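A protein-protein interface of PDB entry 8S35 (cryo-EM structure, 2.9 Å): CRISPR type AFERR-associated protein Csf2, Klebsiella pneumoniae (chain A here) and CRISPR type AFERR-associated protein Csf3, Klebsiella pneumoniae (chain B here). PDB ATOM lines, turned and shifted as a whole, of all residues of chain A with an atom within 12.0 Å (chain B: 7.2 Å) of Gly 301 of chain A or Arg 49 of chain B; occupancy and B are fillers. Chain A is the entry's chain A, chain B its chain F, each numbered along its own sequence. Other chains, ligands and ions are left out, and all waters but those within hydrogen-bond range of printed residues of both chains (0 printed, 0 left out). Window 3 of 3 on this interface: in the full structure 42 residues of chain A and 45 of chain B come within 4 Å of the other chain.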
ATOM      1  N   MET A   1     -22.658  22.285  -6.075  1.00  0.00           N
ATOM      2  CA  MET A   1     -23.399  21.742  -7.247  1.00  0.00           C
ATOM      3  C   MET A   1     -23.905  20.337  -6.952  1.00  0.00           C
ATOM      4  O   MET A   1     -23.289  19.593  -6.192  1.00  0.00           O
ATOM      5  CB  MET A   1     -22.505  21.730  -8.486  1.00  0.00           C
ATOM      6  CG  MET A   1     -22.375  23.083  -9.159  1.00  0.00           C
ATOM      7  SD  MET A   1     -21.747  24.352  -8.043  1.00  0.00           S
ATOM      8  CE  MET A   1     -20.021  23.886  -7.937  1.00  0.00           C
ATOM      9  N   ARG A   2     -25.034  19.982  -7.559  1.00  0.00           N
ATOM     10  CA  ARG A   2     -25.642  18.679  -7.348  1.00  0.00           C
ATOM     11  C   ARG A   2     -26.409  18.281  -8.597  1.00  0.00           C
ATOM     12  O   ARG A   2     -26.898  19.135  -9.342  1.00  0.00           O
ATOM     13  CB  ARG A   2     -26.584  18.683  -6.143  1.00  0.00           C
ATOM     14  CG  ARG A   2     -25.884  18.558  -4.804  1.00  0.00           C
ATOM     15  CD  ARG A   2     -26.889  18.496  -3.669  1.00  0.00           C
ATOM     16  NE  ARG A   2     -27.725  19.690  -3.624  1.00  0.00           N
ATOM     17  CZ  ARG A   2     -28.885  19.780  -2.989  1.00  0.00           C
ATOM     18  NH1 ARG A   2     -29.392  18.757  -2.318  1.00  0.00           N
ATOM     19  NH2 ARG A   2     -29.558  20.926  -3.027  1.00  0.00           N
ATOM     20  N   THR A   3     -26.506  16.973  -8.818  1.00  0.00           N
ATOM     21  CA  THR A   3     -27.268  16.410  -9.924  1.00  0.00           C
ATOM     22  C   THR A   3     -28.578  15.872  -9.362  1.00  0.00           C
ATOM     23  O   THR A   3     -28.583  14.879  -8.629  1.00  0.00           O
ATOM     24  CB  THR A   3     -26.476  15.310 -10.624  1.00  0.00           C
ATOM     25  OG1 THR A   3     -25.149  15.779 -10.887  1.00  0.00           O
ATOM     26  CG2 THR A   3     -27.138  14.909 -11.936  1.00  0.00           C
ATOM     27  N   THR A 297     -30.610  12.371  -5.709  1.00  0.00           N
ATOM     28  CA  THR A 297     -29.293  12.914  -5.995  1.00  0.00           C
ATOM     29  C   THR A 297     -28.285  11.787  -5.868  1.00  0.00           C
ATOM     30  O   THR A 297     -28.608  10.691  -5.410  1.00  0.00           O
ATOM     31  CB  THR A 297     -28.930  14.072  -5.059  1.00  0.00           C
ATOM     32  OG1 THR A 297     -27.690  14.653  -5.477  1.00  0.00           O
ATOM     33  CG2 THR A 297     -28.796  13.587  -3.620  1.00  0.00           C
ATOM     34  N   TRP A 298     -27.054  12.060  -6.274  1.00  0.00           N
ATOM     35  CA  TRP A 298     -25.976  11.089  -6.188  1.00  0.00           C
ATOM     36  C   TRP A 298     -25.128  11.365  -4.956  1.00  0.00           C
ATOM     37  O   TRP A 298     -24.785  12.517  -4.671  1.00  0.00           O
ATOM     38  CB  TRP A 298     -25.114  11.129  -7.445  1.00  0.00           C
ATOM     39  CG  TRP A 298     -25.821  10.599  -8.645  1.00  0.00           C
ATOM     40  CD1 TRP A 298     -26.509  11.320  -9.574  1.00  0.00           C
ATOM     41  CD2 TRP A 298     -25.908   9.231  -9.054  1.00  0.00           C
ATOM     42  NE1 TRP A 298     -27.019  10.486 -10.537  1.00  0.00           N
ATOM     43  CE2 TRP A 298     -26.664   9.198 -10.240  1.00  0.00           C
ATOM     44  CE3 TRP A 298     -25.418   8.032  -8.532  1.00  0.00           C
ATOM     45  CZ2 TRP A 298     -26.945   8.013 -10.910  1.00  0.00           C
ATOM     46  CZ3 TRP A 298     -25.698   6.858  -9.199  1.00  0.00           C
ATOM     47  CH2 TRP A 298     -26.454   6.856 -10.376  1.00  0.00           C
ATOM     48  N   LYS A 299     -24.803  10.306  -4.222  1.00  0.00           N
ATOM     49  CA  LYS A 299     -23.964  10.456  -3.046  1.00  0.00           C
ATOM     50  C   LYS A 299     -22.607  11.017  -3.462  1.00  0.00           C
ATOM     51  O   LYS A 299     -22.108  10.679  -4.542  1.00  0.00           O
ATOM     52  CB  LYS A 299     -23.767   9.109  -2.350  1.00  0.00           C
ATOM     53  CG  LYS A 299     -24.939   8.655  -1.512  1.00  0.00           C
ATOM     54  CD  LYS A 299     -24.584   7.438  -0.676  1.00  0.00           C
ATOM     55  CE  LYS A 299     -24.129   7.836   0.717  1.00  0.00           C
ATOM     56  NZ  LYS A 299     -25.266   8.289   1.566  1.00  0.00           N
ATOM     57  N   PRO A 300     -21.991  11.892  -2.662  1.00  0.00           N
ATOM     58  CA  PRO A 300     -20.634  12.343  -3.003  1.00  0.00           C
ATOM     59  C   PRO A 300     -19.688  11.159  -3.120  1.00  0.00           C
ATOM     60  O   PRO A 300     -19.444  10.438  -2.149  1.00  0.00           O
ATOM     61  CB  PRO A 300     -20.260  13.263  -1.836  1.00  0.00           C
ATOM     62  CG  PRO A 300     -21.550  13.710  -1.271  1.00  0.00           C
ATOM     63  CD  PRO A 300     -22.505  12.577  -1.462  1.00  0.00           C
ATOM     64  N   GLY A 301     -19.163  10.956  -4.318  1.00  0.00           N
ATOM     65  CA  GLY A 301     -18.221   9.866  -4.559  1.00  0.00           C
ATOM     66  C   GLY A 301     -18.858   8.517  -4.809  1.00  0.00           C
ATOM     67  O   GLY A 301     -18.459   7.804  -5.734  1.00  0.00           O
ATOM     68  N   GLU A 302     -19.848   8.145  -4.001  1.00  0.00           N
ATOM     69  CA  GLU A 302     -20.501   6.852  -4.138  1.00  0.00           C
ATOM     70  C   GLU A 302     -21.584   6.906  -5.207  1.00  0.00           C
ATOM     71  O   GLU A 302     -22.314   7.893  -5.326  1.00  0.00           O
ATOM     72  CB  GLU A 302     -21.112   6.418  -2.806  1.00  0.00           C
ATOM     73  CG  GLU A 302     -20.103   6.280  -1.675  1.00  0.00           C
ATOM     74  CD  GLU A 302     -19.837   7.590  -0.955  1.00  0.00           C
ATOM     75  OE1 GLU A 302     -20.809   8.309  -0.639  1.00  0.00           O
ATOM     76  OE2 GLU A 302     -18.655   7.903  -0.708  1.00  0.00           O
ATOM     77  N   LEU A 303     -21.683   5.830  -5.985  1.00  0.00           N
ATOM     78  CA  LEU A 303     -22.721   5.698  -7.008  1.00  0.00           C
ATOM     79  C   LEU A 303     -23.980   5.098  -6.382  1.00  0.00           C
ATOM     80  O   LEU A 303     -24.368   3.960  -6.651  1.00  0.00           O
ATOM     81  CB  LEU A 303     -22.218   4.853  -8.170  1.00  0.00           C
ATOM     82  CG  LEU A 303     -20.937   5.336  -8.855  1.00  0.00           C
ATOM     83  CD1 LEU A 303     -19.695   4.695  -8.242  1.00  0.00           C
ATOM     84  CD2 LEU A 303     -21.000   5.058 -10.345  1.00  0.00           C
ATOM     85  N   VAL A 304     -24.616   5.892  -5.525  1.00  0.00           N
ATOM     86  CA  VAL A 304     -25.844   5.472  -4.852  1.00  0.00           C
ATOM     87  C   VAL A 304     -26.853   6.615  -4.912  1.00  0.00           C
ATOM     88  O   VAL A 304     -26.481   7.768  -4.649  1.00  0.00           O
ATOM     89  CB  VAL A 304     -25.560   5.062  -3.398  1.00  0.00           C
ATOM     90  CG1 VAL A 304     -26.859   4.887  -2.621  1.00  0.00           C
ATOM     91  CG2 VAL A 304     -24.731   3.787  -3.363  1.00  0.00           C
ATOM     92  N   PRO A 305     -28.124   6.367  -5.245  1.00  0.00           N
ATOM     93  CA  PRO A 305     -29.107   7.461  -5.233  1.00  0.00           C
ATOM     94  C   PRO A 305     -29.668   7.702  -3.838  1.00  0.00           C
ATOM     95  O   PRO A 305     -30.256   6.805  -3.231  1.00  0.00           O
ATOM     96  CB  PRO A 305     -30.192   6.967  -6.196  1.00  0.00           C
ATOM     97  CG  PRO A 305     -30.140   5.502  -6.076  1.00  0.00           C
ATOM     98  CD  PRO A 305     -28.701   5.139  -5.825  1.00  0.00           C
ATOM     99  N   VAL A 306     -29.486   8.914  -3.335  1.00  0.00           N
ATOM    100  CA  VAL A 306     -30.174   9.389  -2.141  1.00  0.00           C
ATOM    101  C   VAL A 306     -31.479  10.021  -2.590  1.00  0.00           C
ATOM    102  O   VAL A 306     -31.553  10.601  -3.673  1.00  0.00           O
ATOM    103  CB  VAL A 306     -29.314  10.393  -1.348  1.00  0.00           C
ATOM    104  CG1 VAL A 306     -29.985  10.741  -0.025  1.00  0.00           C
ATOM    105  CG2 VAL A 306     -27.928   9.836  -1.123  1.00  0.00           C
ATOM    106  N   LEU B  34     -21.230   9.618 -15.333  1.00  0.00           N
ATOM    107  CA  LEU B  34     -20.388   9.976 -14.199  1.00  0.00           C
ATOM    108  C   LEU B  34     -20.350  11.483 -13.997  1.00  0.00           C
ATOM    109  O   LEU B  34     -20.360  11.959 -12.857  1.00  0.00           O
ATOM    110  CB  LEU B  34     -18.977   9.433 -14.401  1.00  0.00           C
ATOM    111  CG  LEU B  34     -18.803   7.924 -14.238  1.00  0.00           C
ATOM    112  CD1 LEU B  34     -17.384   7.540 -14.575  1.00  0.00           C
ATOM    113  CD2 LEU B  34     -19.149   7.467 -12.832  1.00  0.00           C
ATOM    114  N   ALA B  37     -23.061  11.952 -12.012  1.00  0.00           N
ATOM    115  CA  ALA B  37     -22.898  11.389 -10.677  1.00  0.00           C
ATOM    116  C   ALA B  37     -21.917  12.206  -9.848  1.00  0.00           C
ATOM    117  O   ALA B  37     -22.207  12.570  -8.704  1.00  0.00           O
ATOM    118  CB  ALA B  37     -22.438   9.935 -10.775  1.00  0.00           C
ATOM    119  N   ILE B  38     -20.753  12.502 -10.411  1.00  0.00           N
ATOM    120  CA  ILE B  38     -19.790  13.405  -9.791  1.00  0.00           C
ATOM    121  C   ILE B  38     -20.129  14.815 -10.268  1.00  0.00           C
ATOM    122  O   ILE B  38     -19.992  15.092 -11.469  1.00  0.00           O
ATOM    123  CB  ILE B  38     -18.351  13.034 -10.161  1.00  0.00           C
ATOM    124  CG1 ILE B  38     -18.086  11.559  -9.849  1.00  0.00           C
ATOM    125  CG2 ILE B  38     -17.361  13.918  -9.409  1.00  0.00           C
ATOM    126  CD1 ILE B  38     -18.138  10.656 -11.059  1.00  0.00           C
ATOM    127  N   PRO B  39     -20.547  15.730  -9.389  1.00  0.00           N
ATOM    128  CA  PRO B  39     -20.968  17.043  -9.892  1.00  0.00           C
ATOM    129  C   PRO B  39     -19.771  17.859 -10.349  1.00  0.00           C
ATOM    130  O   PRO B  39     -19.374  18.839  -9.712  1.00  0.00           O
ATOM    131  CB  PRO B  39     -21.675  17.670  -8.685  1.00  0.00           C
ATOM    132  CG  PRO B  39     -21.015  17.052  -7.515  1.00  0.00           C
ATOM    133  CD  PRO B  39     -20.677  15.646  -7.922  1.00  0.00           C
ATOM    134  N   PRO B  43     -12.868  17.140 -17.404  1.00  0.00           N
ATOM    135  CA  PRO B  43     -12.620  15.808 -17.982  1.00  0.00           C
ATOM    136  C   PRO B  43     -11.661  14.953 -17.176  1.00  0.00           C
ATOM    137  O   PRO B  43     -11.821  13.730 -17.156  1.00  0.00           O
ATOM    138  CB  PRO B  43     -12.056  16.118 -19.378  1.00  0.00           C
ATOM    139  CG  PRO B  43     -11.781  17.575 -19.397  1.00  0.00           C
ATOM    140  CD  PRO B  43     -12.713  18.191 -18.424  1.00  0.00           C
ATOM    141  N   GLY B  44     -10.674  15.551 -16.510  1.00  0.00           N
ATOM    142  CA  GLY B  44      -9.672  14.753 -15.822  1.00  0.00           C
ATOM    143  C   GLY B  44     -10.260  13.864 -14.741  1.00  0.00           C
ATOM    144  O   GLY B  44     -10.031  12.652 -14.722  1.00  0.00           O
ATOM    145  N   VAL B  45     -11.036  14.452 -13.830  1.00  0.00           N
ATOM    146  CA  VAL B  45     -11.554  13.685 -12.701  1.00  0.00           C
ATOM    147  C   VAL B  45     -12.615  12.694 -13.163  1.00  0.00           C
ATOM    148  O   VAL B  45     -12.676  11.558 -12.674  1.00  0.00           O
ATOM    149  CB  VAL B  45     -12.094  14.634 -11.613  1.00  0.00           C
ATOM    150  CG1 VAL B  45     -13.325  15.393 -12.101  1.00  0.00           C
ATOM    151  CG2 VAL B  45     -12.410  13.857 -10.344  1.00  0.00           C
ATOM    152  N   VAL B  46     -13.465  13.098 -14.109  1.00  0.00           N
ATOM    153  CA  VAL B  46     -14.493  12.186 -14.602  1.00  0.00           C
ATOM    154  C   VAL B  46     -13.844  11.008 -15.311  1.00  0.00           C
ATOM    155  O   VAL B  46     -14.316   9.871 -15.217  1.00  0.00           O
ATOM    156  CB  VAL B  46     -15.483  12.931 -15.517  1.00  0.00           C
ATOM    157  CG1 VAL B  46     -16.611  12.004 -15.963  1.00  0.00           C
ATOM    158  CG2 VAL B  46     -16.061  14.145 -14.806  1.00  0.00           C
ATOM    159  N   LEU B  47     -12.751  11.258 -16.031  1.00  0.00           N
ATOM    160  CA  LEU B  47     -12.027  10.169 -16.676  1.00  0.00           C
ATOM    161  C   LEU B  47     -11.388   9.255 -15.642  1.00  0.00           C
ATOM    162  O   LEU B  47     -11.459   8.027 -15.763  1.00  0.00           O
ATOM    163  CB  LEU B  47     -10.962  10.726 -17.620  1.00  0.00           C
ATOM    164  CG  LEU B  47     -11.327  10.919 -19.097  1.00  0.00           C
ATOM    165  CD1 LEU B  47     -11.524   9.572 -19.769  1.00  0.00           C
ATOM    166  CD2 LEU B  47     -12.551  11.816 -19.307  1.00  0.00           C
ATOM    167  N   ALA B  48     -10.754   9.839 -14.624  1.00  0.00           N
ATOM    168  CA  ALA B  48     -10.124   9.032 -13.585  1.00  0.00           C
ATOM    169  C   ALA B  48     -11.144   8.133 -12.904  1.00  0.00           C
ATOM    170  O   ALA B  48     -10.848   6.975 -12.586  1.00  0.00           O
ATOM    171  CB  ALA B  48      -9.438   9.935 -12.563  1.00  0.00           C
ATOM    172  N   ARG B  49     -12.355   8.643 -12.677  1.00  0.00           N
ATOM    173  CA  ARG B  49     -13.391   7.801 -12.092  1.00  0.00           C
ATOM    174  C   ARG B  49     -13.945   6.814 -13.111  1.00  0.00           C
ATOM    175  O   ARG B  49     -14.413   5.734 -12.734  1.00  0.00           O
ATOM    176  CB  ARG B  49     -14.520   8.662 -11.527  1.00  0.00           C
ATOM    177  CG  ARG B  49     -14.390   8.957 -10.040  1.00  0.00           C
ATOM    178  CD  ARG B  49     -14.751   7.752  -9.183  1.00  0.00           C
ATOM    179  NE  ARG B  49     -16.157   7.387  -9.310  1.00  0.00           N
ATOM    180  CZ  ARG B  49     -17.162   8.044  -8.743  1.00  0.00           C
ATOM    181  NH1 ARG B  49     -16.957   9.114  -7.992  1.00  0.00           N
ATOM    182  NH2 ARG B  49     -18.406   7.615  -8.935  1.00  0.00           N
ATOM    183  N   LEU B  50     -13.893   7.159 -14.398  1.00  0.00           N
ATOM    184  CA  LEU B  50     -14.373   6.246 -15.429  1.00  0.00           C
ATOM    185  C   LEU B  50     -13.438   5.059 -15.587  1.00  0.00           C
ATOM    186  O   LEU B  50     -13.887   3.936 -15.848  1.00  0.00           O
ATOM    187  CB  LEU B  50     -14.527   6.997 -16.751  1.00  0.00           C
ATOM    188  CG  LEU B  50     -15.148   6.252 -17.933  1.00  0.00           C
ATOM    189  CD1 LEU B  50     -16.485   5.640 -17.566  1.00  0.00           C
ATOM    190  CD2 LEU B  50     -15.311   7.196 -19.110  1.00  0.00           C
ATOM    191  N   LYS B  51     -12.134   5.282 -15.424  1.00  0.00           N
ATOM    192  CA  LYS B  51     -11.183   4.181 -15.464  1.00  0.00           C
ATOM    193  C   LYS B  51     -11.426   3.188 -14.340  1.00  0.00           C
ATOM    194  O   LYS B  51     -11.057   2.016 -14.471  1.00  0.00           O
ATOM    195  CB  LYS B  51      -9.755   4.719 -15.393  1.00  0.00           C
ATOM    196  CG  LYS B  51      -9.288   5.381 -16.676  1.00  0.00           C
ATOM    197  CD  LYS B  51      -7.932   6.037 -16.505  1.00  0.00           C
ATOM    198  CE  LYS B  51      -7.587   6.906 -17.701  1.00  0.00           C
ATOM    199  NZ  LYS B  51      -8.328   8.196 -17.678  1.00  0.00           N
ATOM    200  N   GLU B  52     -12.042   3.627 -13.243  1.00  0.00           N
ATOM    201  CA  GLU B  52     -12.313   2.744 -12.120  1.00  0.00           C
ATOM    202  C   GLU B  52     -13.494   1.818 -12.378  1.00  0.00           C
ATOM    203  O   GLU B  52     -13.619   0.798 -11.694  1.00  0.00           O
ATOM    204  CB  GLU B  52     -12.568   3.577 -10.862  1.00  0.00           C
ATOM    205  CG  GLU B  52     -12.657   2.765  -9.571  1.00  0.00           C
ATOM    206  CD  GLU B  52     -14.072   2.336  -9.209  1.00  0.00           C
ATOM    207  OE1 GLU B  52     -15.039   2.807  -9.845  1.00  0.00           O
ATOM    208  OE2 GLU B  52     -14.218   1.516  -8.278  1.00  0.00           O
ATOM    209  N   ILE B  53     -14.353   2.145 -13.346  1.00  0.00           N
ATOM    210  CA  ILE B  53     -15.481   1.293 -13.711  1.00  0.00           C
ATOM    211  C   ILE B  53     -15.345   0.700 -15.103  1.00  0.00           C
ATOM    212  O   ILE B  53     -16.175  -0.145 -15.480  1.00  0.00           O
ATOM    213  CB  ILE B  53     -16.820   2.053 -13.596  1.00  0.00           C
ATOM    214  CG1 ILE B  53     -16.840   3.291 -14.501  1.00  0.00           C
ATOM    215  CG2 ILE B  53     -17.059   2.471 -12.158  1.00  0.00           C
ATOM    216  CD1 ILE B  53     -18.216   3.898 -14.656  1.00  0.00           C
ATOM    217  N   LEU B  54     -14.342   1.106 -15.878  1.00  0.00           N
ATOM    218  CA  LEU B  54     -14.133   0.614 -17.230  1.00  0.00           C
ATOM    219  C   LEU B  54     -12.662   0.291 -17.421  1.00  0.00           C
ATOM    220  O   LEU B  54     -11.794   0.999 -16.902  1.00  0.00           O
ATOM    221  CB  LEU B  54     -14.570   1.645 -18.276  1.00  0.00           C
ATOM    222  CG  LEU B  54     -15.923   1.444 -18.954  1.00  0.00           C
ATOM    223  CD1 LEU B  54     -16.248   2.661 -19.804  1.00  0.00           C
ATOM    224  CD2 LEU B  54     -15.933   0.186 -19.797  1.00  0.00           C
ATOM    225  N   PHE B  63     -11.113   3.248 -23.942  1.00  0.00           N
ATOM    226  CA  PHE B  63     -11.810   2.402 -22.989  1.00  0.00           C
ATOM    227  C   PHE B  63     -12.356   1.166 -23.687  1.00  0.00           C
ATOM    228  O   PHE B  63     -12.702   1.198 -24.870  1.00  0.00           O
ATOM    229  CB  PHE B  63     -12.962   3.159 -22.330  1.00  0.00           C
ATOM    230  CG  PHE B  63     -12.526   4.155 -21.303  1.00  0.00           C
ATOM    231  CD1 PHE B  63     -11.913   3.743 -20.134  1.00  0.00           C
ATOM    232  CD2 PHE B  63     -12.738   5.504 -21.502  1.00  0.00           C
ATOM    233  CE1 PHE B  63     -11.516   4.662 -19.188  1.00  0.00           C
ATOM    234  CE2 PHE B  63     -12.344   6.424 -20.560  1.00  0.00           C
ATOM    235  CZ  PHE B  63     -11.732   6.004 -19.401  1.00  0.00           C
ATOM    236  N   LEU B 147     -25.495   3.302 -13.212  1.00  0.00           N
ATOM    237  CA  LEU B 147     -25.440   4.522 -14.005  1.00  0.00           C
ATOM    238  C   LEU B 147     -26.503   4.516 -15.094  1.00  0.00           C
ATOM    239  O   LEU B 147     -27.303   5.451 -15.201  1.00  0.00           O
ATOM    240  CB  LEU B 147     -24.046   4.682 -14.610  1.00  0.00           C
ATOM    241  CG  LEU B 147     -22.928   5.053 -13.634  1.00  0.00           C
ATOM    242  CD1 LEU B 147     -21.583   5.007 -14.334  1.00  0.00           C
ATOM    243  CD2 LEU B 147     -23.159   6.421 -13.014  1.00  0.00           C
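NH1 of Arg 49 of chain B is in hydrogen-bond range of O of Gly 301 of chain A (3.0 Å).
Met 1 of chain A touches Pro 39 of chain B.
Ala 37 of chain B touches Trp 298 of chain A.
CD2 of Leu 303 of chain A touches CD2 of Leu 34 of chain B, 3.9 Å away.
Leu 303 of chain A touches Arg 49 of chain B.
CD2 of Leu 147 of chain B touches CD2 of Leu 303 of chain A, at 3.7 Å.
Printed residues of chain B within 4 Å of Met 1 of chain A: Pro 39.
Thr 3 of chain A touches none of the printed residues of chain B.
Of the printed residues of chain B, Trp 298 of chain A touches Ala 37.
Gly 301 of chain A touches one residue of chain B.
Glu 302 of chain A touches none of the printed residues of chain B.
Printed residues of chain B within 4 Å of Leu 303 of chain A: Leu 34, Arg 49 and Leu 147.
Leu 34 of chain B touches just one residue of chain A: Leu 303.
No residue of chain A comes within 4 Å of Ile 38 of chain B.
Printed residues of chain A within 4 Å of Pro 39 of chain B: Met 1 (3.5 Å).
No residue of chain A comes within 4 Å of Val 45 of chain B.
No residue of chain A comes within 4 Å of Val 46 of chain B.
No residue of chain A comes within 4 Å of Leu 47 of chain B.
Arg 49 of chain B touches two residues of chain A.
No residue of chain A comes within 4 Å of Leu 50 of chain B.
No residue of chain A comes within 4 Å of Lys 51 of chain B.
No residue of chain A comes within 4 Å of Glu 52 of chain B.
No residue of chain A comes within 4 Å of Ile 53 of chain B.
Of the printed residues of chain A, Leu 147 of chain B touches Leu 303 (3.7 Å).
The nearest printed residue of chain B that does not touch Gly 301 of chain A is Ile 38 of chain B (5.6 Å).
The nearest residue of chain A that does not touch Arg 49 of chain B is Glu 302 of chain A (4.9 Å).
The nearest printed residue of chain B that does not touch Met 1 of chain A is Ile 38 of chain B (7.0 Å).
Printed residues of chain A that touch a printed residue of chain B: Met 1, Trp 298, Gly 301 and Leu 303.
Hydrophobic or aromatic side chains of chain A within 4 Å of the printed part of chain B: Trp 298 and Leu 303.
Hydrophobic or aromatic side chains of chain B that line the printed part of chain A: Leu 34, Ala 37, Pro 39 and Leu 147.
Among the printed residues, 6 pairs touch across the chains.
Among the printed residues, no Asp or Glu carboxylate lies within 4 Å of a Lys or Arg side-chain nitrogen of the other chain.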
